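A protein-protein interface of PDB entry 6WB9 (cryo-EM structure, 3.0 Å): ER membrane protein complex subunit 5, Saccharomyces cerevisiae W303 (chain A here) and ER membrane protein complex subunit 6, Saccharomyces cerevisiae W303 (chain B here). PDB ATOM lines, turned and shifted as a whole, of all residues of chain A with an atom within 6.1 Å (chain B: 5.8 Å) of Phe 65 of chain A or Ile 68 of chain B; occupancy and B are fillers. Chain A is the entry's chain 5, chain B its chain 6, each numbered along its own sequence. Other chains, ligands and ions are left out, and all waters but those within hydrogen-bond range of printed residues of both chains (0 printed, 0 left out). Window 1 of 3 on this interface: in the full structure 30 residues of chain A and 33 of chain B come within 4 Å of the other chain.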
ATOM      1  N   PHE A  60     -18.758  28.842  19.835  1.00  0.00           N
ATOM      2  CA  PHE A  60     -19.838  29.237  20.737  1.00  0.00           C
ATOM      3  C   PHE A  60     -21.030  28.297  20.619  1.00  0.00           C
ATOM      4  O   PHE A  60     -21.683  27.994  21.623  1.00  0.00           O
ATOM      5  CB  PHE A  60     -20.276  30.675  20.463  1.00  0.00           C
ATOM      6  CG  PHE A  60     -21.254  31.209  21.477  1.00  0.00           C
ATOM      7  CD1 PHE A  60     -20.800  31.774  22.655  1.00  0.00           C
ATOM      8  CD2 PHE A  60     -22.625  31.144  21.255  1.00  0.00           C
ATOM      9  CE1 PHE A  60     -21.688  32.261  23.588  1.00  0.00           C
ATOM     10  CE2 PHE A  60     -23.514  31.620  22.188  1.00  0.00           C
ATOM     11  CZ  PHE A  60     -23.046  32.184  23.353  1.00  0.00           C
ATOM     12  N   VAL A  61     -21.344  27.850  19.401  1.00  0.00           N
ATOM     13  CA  VAL A  61     -22.438  26.902  19.215  1.00  0.00           C
ATOM     14  C   VAL A  61     -22.105  25.565  19.872  1.00  0.00           C
ATOM     15  O   VAL A  61     -22.951  24.959  20.544  1.00  0.00           O
ATOM     16  CB  VAL A  61     -22.745  26.766  17.711  1.00  0.00           C
ATOM     17  CG1 VAL A  61     -23.566  25.531  17.411  1.00  0.00           C
ATOM     18  CG2 VAL A  61     -23.478  27.999  17.227  1.00  0.00           C
ATOM     19  N   LEU A  62     -20.849  25.126  19.759  1.00  0.00           N
ATOM     20  CA  LEU A  62     -20.418  23.918  20.451  1.00  0.00           C
ATOM     21  C   LEU A  62     -20.375  24.109  21.962  1.00  0.00           C
ATOM     22  O   LEU A  62     -20.579  23.148  22.704  1.00  0.00           O
ATOM     23  CB  LEU A  62     -19.051  23.473  19.942  1.00  0.00           C
ATOM     24  CG  LEU A  62     -19.006  22.901  18.528  1.00  0.00           C
ATOM     25  CD1 LEU A  62     -17.587  22.506  18.177  1.00  0.00           C
ATOM     26  CD2 LEU A  62     -19.945  21.719  18.407  1.00  0.00           C
ATOM     27  N   ALA A  63     -20.120  25.328  22.439  1.00  0.00           N
ATOM     28  CA  ALA A  63     -20.157  25.573  23.875  1.00  0.00           C
ATOM     29  C   ALA A  63     -21.581  25.583  24.407  1.00  0.00           C
ATOM     30  O   ALA A  63     -21.815  25.198  25.556  1.00  0.00           O
ATOM     31  CB  ALA A  63     -19.472  26.893  24.198  1.00  0.00           C
ATOM     32  N   VAL A  64     -22.534  26.046  23.599  1.00  0.00           N
ATOM     33  CA  VAL A  64     -23.937  25.999  23.995  1.00  0.00           C
ATOM     34  C   VAL A  64     -24.435  24.559  24.012  1.00  0.00           C
ATOM     35  O   VAL A  64     -25.094  24.128  24.965  1.00  0.00           O
ATOM     36  CB  VAL A  64     -24.777  26.894  23.065  1.00  0.00           C
ATOM     37  CG1 VAL A  64     -26.257  26.601  23.197  1.00  0.00           C
ATOM     38  CG2 VAL A  64     -24.521  28.344  23.383  1.00  0.00           C
ATOM     39  N   PHE A  65     -24.089  23.777  22.989  1.00  0.00           N
ATOM     40  CA  PHE A  65     -24.625  22.425  22.897  1.00  0.00           C
ATOM     41  C   PHE A  65     -23.899  21.420  23.781  1.00  0.00           C
ATOM     42  O   PHE A  65     -24.497  20.402  24.142  1.00  0.00           O
ATOM     43  CB  PHE A  65     -24.615  21.954  21.447  1.00  0.00           C
ATOM     44  CG  PHE A  65     -25.730  22.525  20.633  1.00  0.00           C
ATOM     45  CD1 PHE A  65     -27.040  22.289  20.986  1.00  0.00           C
ATOM     46  CD2 PHE A  65     -25.471  23.305  19.525  1.00  0.00           C
ATOM     47  CE1 PHE A  65     -28.070  22.818  20.251  1.00  0.00           C
ATOM     48  CE2 PHE A  65     -26.500  23.837  18.784  1.00  0.00           C
ATOM     49  CZ  PHE A  65     -27.801  23.590  19.147  1.00  0.00           C
ATOM     50  N   THR A  66     -22.644  21.662  24.145  1.00  0.00           N
ATOM     51  CA  THR A  66     -21.984  20.808  25.124  1.00  0.00           C
ATOM     52  C   THR A  66     -22.194  21.283  26.553  1.00  0.00           C
ATOM     53  O   THR A  66     -21.627  20.692  27.475  1.00  0.00           O
ATOM     54  CB  THR A  66     -20.482  20.697  24.842  1.00  0.00           C
ATOM     55  OG1 THR A  66     -19.909  22.005  24.761  1.00  0.00           O
ATOM     56  CG2 THR A  66     -20.238  19.960  23.538  1.00  0.00           C
ATOM     57  N   SER A  67     -22.990  22.335  26.761  1.00  0.00           N
ATOM     58  CA  SER A  67     -23.434  22.664  28.108  1.00  0.00           C
ATOM     59  C   SER A  67     -24.496  21.696  28.591  1.00  0.00           C
ATOM     60  O   SER A  67     -24.685  21.547  29.801  1.00  0.00           O
ATOM     61  CB  SER A  67     -23.969  24.094  28.162  1.00  0.00           C
ATOM     62  OG  SER A  67     -25.170  24.218  27.424  1.00  0.00           O
ATOM     63  N   PHE A  68     -25.186  21.039  27.666  1.00  0.00           N
ATOM     64  CA  PHE A  68     -26.169  20.016  27.990  1.00  0.00           C
ATOM     65  C   PHE A  68     -25.437  18.747  28.384  1.00  0.00           C
ATOM     66  O   PHE A  68     -24.834  18.082  27.537  1.00  0.00           O
ATOM     67  CB  PHE A  68     -27.080  19.743  26.799  1.00  0.00           C
ATOM     68  CG  PHE A  68     -28.100  20.805  26.549  1.00  0.00           C
ATOM     69  CD1 PHE A  68     -29.429  20.589  26.865  1.00  0.00           C
ATOM     70  CD2 PHE A  68     -27.738  22.009  25.981  1.00  0.00           C
ATOM     71  CE1 PHE A  68     -30.371  21.562  26.628  1.00  0.00           C
ATOM     72  CE2 PHE A  68     -28.666  22.978  25.753  1.00  0.00           C
ATOM     73  CZ  PHE A  68     -29.988  22.759  26.069  1.00  0.00           C
ATOM     74  N   GLU A  69     -25.481  18.410  29.662  1.00  0.00           N
ATOM     75  CA  GLU A  69     -25.015  17.113  30.108  1.00  0.00           C
ATOM     76  C   GLU A  69     -26.188  16.146  30.112  1.00  0.00           C
ATOM     77  O   GLU A  69     -27.343  16.550  30.268  1.00  0.00           O
ATOM     78  CB  GLU A  69     -24.392  17.213  31.498  1.00  0.00           C
ATOM     79  CG  GLU A  69     -23.356  18.315  31.601  1.00  0.00           C
ATOM     80  CD  GLU A  69     -22.815  18.486  32.999  1.00  0.00           C
ATOM     81  OE1 GLU A  69     -22.560  17.465  33.669  1.00  0.00           O
ATOM     82  OE2 GLU A  69     -22.653  19.646  33.429  1.00  0.00           O
ATOM     83  N   ASN A  88     -30.687  10.683  28.258  1.00  0.00           N
ATOM     84  CA  ASN A  88     -31.389  11.808  27.663  1.00  0.00           C
ATOM     85  C   ASN A  88     -30.731  13.118  28.074  1.00  0.00           C
ATOM     86  O   ASN A  88     -30.166  13.231  29.164  1.00  0.00           O
ATOM     87  CB  ASN A  88     -32.860  11.824  28.081  1.00  0.00           C
ATOM     88  CG  ASN A  88     -33.626  10.627  27.568  1.00  0.00           C
ATOM     89  OD1 ASN A  88     -33.237  10.001  26.585  1.00  0.00           O
ATOM     90  ND2 ASN A  88     -34.730  10.310  28.226  1.00  0.00           N
ATOM     91  N   TYR A  89     -30.803  14.106  27.186  1.00  0.00           N
ATOM     92  CA  TYR A  89     -30.365  15.455  27.520  1.00  0.00           C
ATOM     93  C   TYR A  89     -31.489  16.291  28.102  1.00  0.00           C
ATOM     94  O   TYR A  89     -31.234  17.177  28.925  1.00  0.00           O
ATOM     95  CB  TYR A  89     -29.807  16.164  26.285  1.00  0.00           C
ATOM     96  CG  TYR A  89     -28.485  15.631  25.798  1.00  0.00           C
ATOM     97  CD1 TYR A  89     -27.302  15.986  26.424  1.00  0.00           C
ATOM     98  CD2 TYR A  89     -28.420  14.786  24.704  1.00  0.00           C
ATOM     99  CE1 TYR A  89     -26.091  15.508  25.980  1.00  0.00           C
ATOM    100  CE2 TYR A  89     -27.213  14.299  24.252  1.00  0.00           C
ATOM    101  CZ  TYR A  89     -26.054  14.665  24.894  1.00  0.00           C
ATOM    102  OH  TYR A  89     -24.847  14.185  24.449  1.00  0.00           O
ATOM    103  N   LEU A  90     -32.721  16.027  27.686  1.00  0.00           N
ATOM    104  CA  LEU A  90     -33.903  16.724  28.157  1.00  0.00           C
ATOM    105  C   LEU A  90     -34.780  15.767  28.951  1.00  0.00           C
ATOM    106  O   LEU A  90     -34.539  14.560  29.008  1.00  0.00           O
ATOM    107  CB  LEU A  90     -34.687  17.312  26.983  1.00  0.00           C
ATOM    108  CG  LEU A  90     -33.895  18.205  26.034  1.00  0.00           C
ATOM    109  CD1 LEU A  90     -34.683  18.450  24.777  1.00  0.00           C
ATOM    110  CD2 LEU A  90     -33.542  19.516  26.703  1.00  0.00           C
ATOM    111  N   VAL B  27     -30.928  28.075  24.382  1.00  0.00           N
ATOM    112  CA  VAL B  27     -30.201  27.814  23.137  1.00  0.00           C
ATOM    113  C   VAL B  27     -30.522  28.875  22.095  1.00  0.00           C
ATOM    114  O   VAL B  27     -29.621  29.462  21.484  1.00  0.00           O
ATOM    115  CB  VAL B  27     -30.522  26.405  22.611  1.00  0.00           C
ATOM    116  CG1 VAL B  27     -30.055  26.239  21.178  1.00  0.00           C
ATOM    117  CG2 VAL B  27     -29.870  25.386  23.472  1.00  0.00           C
ATOM    118  N   SER B  31     -27.975  31.753  20.736  1.00  0.00           N
ATOM    119  CA  SER B  31     -27.703  31.642  19.312  1.00  0.00           C
ATOM    120  C   SER B  31     -28.086  32.912  18.571  1.00  0.00           C
ATOM    121  O   SER B  31     -27.327  33.375  17.721  1.00  0.00           O
ATOM    122  CB  SER B  31     -28.445  30.440  18.740  1.00  0.00           C
ATOM    123  OG  SER B  31     -28.085  29.264  19.442  1.00  0.00           O
ATOM    124  N   ILE B  60     -28.972  25.801  13.654  1.00  0.00           N
ATOM    125  CA  ILE B  60     -28.780  25.569  15.083  1.00  0.00           C
ATOM    126  C   ILE B  60     -29.969  24.809  15.669  1.00  0.00           C
ATOM    127  O   ILE B  60     -29.796  23.920  16.509  1.00  0.00           O
ATOM    128  CB  ILE B  60     -28.519  26.913  15.792  1.00  0.00           C
ATOM    129  CG1 ILE B  60     -27.092  27.374  15.511  1.00  0.00           C
ATOM    130  CG2 ILE B  60     -28.732  26.829  17.288  1.00  0.00           C
ATOM    131  CD1 ILE B  60     -26.858  28.829  15.787  1.00  0.00           C
ATOM    132  N   ASN B  61     -31.183  25.098  15.191  1.00  0.00           N
ATOM    133  CA  ASN B  61     -32.350  24.323  15.618  1.00  0.00           C
ATOM    134  C   ASN B  61     -32.283  22.874  15.135  1.00  0.00           C
ATOM    135  O   ASN B  61     -32.701  21.954  15.850  1.00  0.00           O
ATOM    136  CB  ASN B  61     -33.633  24.987  15.126  1.00  0.00           C
ATOM    137  CG  ASN B  61     -33.961  26.256  15.879  1.00  0.00           C
ATOM    138  OD1 ASN B  61     -33.554  26.434  17.025  1.00  0.00           O
ATOM    139  ND2 ASN B  61     -34.706  27.145  15.240  1.00  0.00           N
ATOM    140  N   ILE B  63     -29.433  21.222  14.608  1.00  0.00           N
ATOM    141  CA  ILE B  63     -28.422  20.624  15.480  1.00  0.00           C
ATOM    142  C   ILE B  63     -28.998  20.365  16.872  1.00  0.00           C
ATOM    143  O   ILE B  63     -28.620  19.396  17.539  1.00  0.00           O
ATOM    144  CB  ILE B  63     -27.165  21.523  15.508  1.00  0.00           C
ATOM    145  CG1 ILE B  63     -26.504  21.547  14.132  1.00  0.00           C
ATOM    146  CG2 ILE B  63     -26.117  21.041  16.494  1.00  0.00           C
ATOM    147  CD1 ILE B  63     -25.364  22.526  14.027  1.00  0.00           C
ATOM    148  N   TYR B  64     -29.963  21.176  17.306  1.00  0.00           N
ATOM    149  CA  TYR B  64     -30.645  20.915  18.570  1.00  0.00           C
ATOM    150  C   TYR B  64     -31.521  19.673  18.485  1.00  0.00           C
ATOM    151  O   TYR B  64     -31.613  18.908  19.450  1.00  0.00           O
ATOM    152  CB  TYR B  64     -31.476  22.129  18.978  1.00  0.00           C
ATOM    153  CG  TYR B  64     -32.081  22.027  20.359  1.00  0.00           C
ATOM    154  CD1 TYR B  64     -31.336  22.349  21.486  1.00  0.00           C
ATOM    155  CD2 TYR B  64     -33.397  21.621  20.537  1.00  0.00           C
ATOM    156  CE1 TYR B  64     -31.881  22.258  22.746  1.00  0.00           C
ATOM    157  CE2 TYR B  64     -33.947  21.527  21.796  1.00  0.00           C
ATOM    158  CZ  TYR B  64     -33.183  21.847  22.894  1.00  0.00           C
ATOM    159  OH  TYR B  64     -33.730  21.759  24.149  1.00  0.00           O
ATOM    160  N   ILE B  65     -32.183  19.463  17.346  1.00  0.00           N
ATOM    161  CA  ILE B  65     -33.010  18.268  17.185  1.00  0.00           C
ATOM    162  C   ILE B  65     -32.139  17.019  17.072  1.00  0.00           C
ATOM    163  O   ILE B  65     -32.467  15.962  17.626  1.00  0.00           O
ATOM    164  CB  ILE B  65     -33.948  18.438  15.974  1.00  0.00           C
ATOM    165  CG1 ILE B  65     -34.937  19.566  16.242  1.00  0.00           C
ATOM    166  CG2 ILE B  65     -34.706  17.155  15.659  1.00  0.00           C
ATOM    167  CD1 ILE B  65     -35.980  19.736  15.179  1.00  0.00           C
ATOM    168  N   VAL B  66     -30.991  17.132  16.408  1.00  0.00           N
ATOM    169  CA  VAL B  66     -30.129  15.971  16.205  1.00  0.00           C
ATOM    170  C   VAL B  66     -29.362  15.626  17.479  1.00  0.00           C
ATOM    171  O   VAL B  66     -29.343  14.470  17.914  1.00  0.00           O
ATOM    172  CB  VAL B  66     -29.182  16.219  15.017  1.00  0.00           C
ATOM    173  CG1 VAL B  66     -28.096  15.164  14.958  1.00  0.00           C
ATOM    174  CG2 VAL B  66     -29.967  16.226  13.720  1.00  0.00           C
ATOM    175  N   TRP B  67     -28.732  16.614  18.107  1.00  0.00           N
ATOM    176  CA  TRP B  67     -27.828  16.359  19.219  1.00  0.00           C
ATOM    177  C   TRP B  67     -28.546  16.312  20.563  1.00  0.00           C
ATOM    178  O   TRP B  67     -28.314  15.395  21.355  1.00  0.00           O
ATOM    179  CB  TRP B  67     -26.722  17.420  19.243  1.00  0.00           C
ATOM    180  CG  TRP B  67     -25.630  17.153  20.239  1.00  0.00           C
ATOM    181  CD1 TRP B  67     -25.318  17.908  21.327  1.00  0.00           C
ATOM    182  CD2 TRP B  67     -24.707  16.055  20.237  1.00  0.00           C
ATOM    183  NE1 TRP B  67     -24.263  17.357  22.004  1.00  0.00           N
ATOM    184  CE2 TRP B  67     -23.867  16.215  21.357  1.00  0.00           C
ATOM    185  CE3 TRP B  67     -24.505  14.953  19.396  1.00  0.00           C
ATOM    186  CZ2 TRP B  67     -22.844  15.315  21.660  1.00  0.00           C
ATOM    187  CZ3 TRP B  67     -23.491  14.060  19.699  1.00  0.00           C
ATOM    188  CH2 TRP B  67     -22.674  14.246  20.822  1.00  0.00           C
ATOM    189  N   ILE B  68     -29.413  17.280  20.839  1.00  0.00           N
ATOM    190  CA  ILE B  68     -30.055  17.369  22.150  1.00  0.00           C
ATOM    191  C   ILE B  68     -31.332  16.547  22.200  1.00  0.00           C
ATOM    192  O   ILE B  68     -31.524  15.735  23.109  1.00  0.00           O
ATOM    193  CB  ILE B  68     -30.324  18.841  22.514  1.00  0.00           C
ATOM    194  CG1 ILE B  68     -29.043  19.655  22.412  1.00  0.00           C
ATOM    195  CG2 ILE B  68     -30.884  18.936  23.907  1.00  0.00           C
ATOM    196  CD1 ILE B  68     -27.954  19.170  23.299  1.00  0.00           C
ATOM    197  N   CYS B  69     -32.228  16.737  21.232  1.00  0.00           N
ATOM    198  CA  CYS B  69     -33.453  15.950  21.184  1.00  0.00           C
ATOM    199  C   CYS B  69     -33.220  14.520  20.717  1.00  0.00           C
ATOM    200  O   CYS B  69     -34.142  13.706  20.830  1.00  0.00           O
ATOM    201  CB  CYS B  69     -34.477  16.625  20.274  1.00  0.00           C
ATOM    202  SG  CYS B  69     -35.068  18.214  20.865  1.00  0.00           S
ATOM    203  N   GLN B  70     -32.028  14.221  20.183  1.00  0.00           N
ATOM    204  CA  GLN B  70     -31.585  12.872  19.808  1.00  0.00           C
ATOM    205  C   GLN B  70     -32.497  12.243  18.755  1.00  0.00           C
ATOM    206  O   GLN B  70     -32.940  11.101  18.889  1.00  0.00           O
ATOM    207  CB  GLN B  70     -31.449  11.977  21.041  1.00  0.00           C
ATOM    208  CG  GLN B  70     -30.355  12.429  21.983  1.00  0.00           C
ATOM    209  CD  GLN B  70     -30.455  11.789  23.343  1.00  0.00           C
ATOM    210  OE1 GLN B  70     -29.458  11.653  24.049  1.00  0.00           O
ATOM    211  NE2 GLN B  70     -31.662  11.400  23.726  1.00  0.00           N
ATOM    212  N   PHE B  76     -39.891  15.196  23.879  1.00  0.00           N
ATOM    213  CA  PHE B  76     -39.402  16.315  24.662  1.00  0.00           C
ATOM    214  C   PHE B  76     -40.173  17.602  24.428  1.00  0.00           C
ATOM    215  O   PHE B  76     -40.126  18.489  25.285  1.00  0.00           O
ATOM    216  CB  PHE B  76     -37.920  16.567  24.354  1.00  0.00           C
ATOM    217  CG  PHE B  76     -37.048  15.373  24.577  1.00  0.00           C
ATOM    218  CD1 PHE B  76     -37.153  14.634  25.739  1.00  0.00           C
ATOM    219  CD2 PHE B  76     -36.129  14.982  23.622  1.00  0.00           C
ATOM    220  CE1 PHE B  76     -36.350  13.534  25.951  1.00  0.00           C
ATOM    221  CE2 PHE B  76     -35.324  13.881  23.830  1.00  0.00           C
ATOM    222  CZ  PHE B  76     -35.436  13.159  24.995  1.00  0.00           C
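The backbone carbonyl oxygen of Val 27 of chain B is in hydrogen-bond range of the side-chain hydroxyl of Ser 31 of chain B, at 2.6 Å. O of Ile 65 of chain B is in hydrogen-bond range of N of Gln 70 of chain B. O of Tyr 64 of chain B is in hydrogen-bond range of N of Cys 69 of chain B. The backbone carbonyl oxygen (O) of Val 64 of chain A is in hydrogen-bond range of the side-chain hydroxyl (OG) of Ser 67 of chain A (2.5 Å).
Phe 65 of chain A touches five residues of chain B. Of chain A, only Phe 65, Phe 68, Tyr 89 and Leu 90 come within 4 Å of Ile 68 of chain B. Of the printed residues of chain B, Phe 68 of chain A touches Val 27, Tyr 64 and Ile 68. Printed residues of chain A within 4 Å of Val 27 of chain B: Val 64 and Phe 68. Of the printed residues of chain A, Gln 70 of chain B touches Asn 88 (3.6 Å) and Tyr 89 (3.4 Å). Asn 61 of chain B touches none of the printed residues of chain A. The nearest residue of chain B that does not touch Phe 65 of chain A is Val 27 of chain B (4.03 Å). The nearest residue of chain A that does not touch Ile 68 of chain B is Asn 88 of chain A (5.7 Å). The nearest printed residue of chain A that does not touch Gln 70 of chain B is Leu 90 of chain A (6.2 Å).
Of the 13 printed residues of chain B, 9 touch a printed residue of chain A. Of the 13 printed residues of chain A, 7 touch a printed residue of chain B. Among the printed residues, no Asp or Glu carboxylate lies within 4 Å of a Lys or Arg side-chain nitrogen of the other chain.
Among the printed residues, merely in contact across the chains: Val 61 of chain A with Ile 60 of chain B, Val 64 of chain A with Val 27 of chain B, Phe 65 of chain A with Ile 60 of chain B, Phe 65 of chain A with Ile 63 of chain B, Phe 65 of chain A with Tyr 64 of chain B, Phe 65 of chain A with Trp 67 of chain B, Phe 65 of chain A with Ile 68 of chain B, Phe 68 of chain A with Val 27 of chain B, Phe 68 of chain A with Tyr 64 of chain B, Phe 68 of chain A with Ile 68 of chain B, Asn 88 of chain A with Gln 70 of chain B, Tyr 89 of chain A with Trp 67 of chain B, Tyr 89 of chain A with Ile 68 of chain B, Tyr 89 of chain A with Gln 70 of chain B, Leu 90 of chain A with Tyr 64 of chain B, Leu 90 of chain A with Ile 68 of chain B, Leu 90 of chain A with Cys 69 of chain B and Leu 90 of chain A with Phe 76 of chain B.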
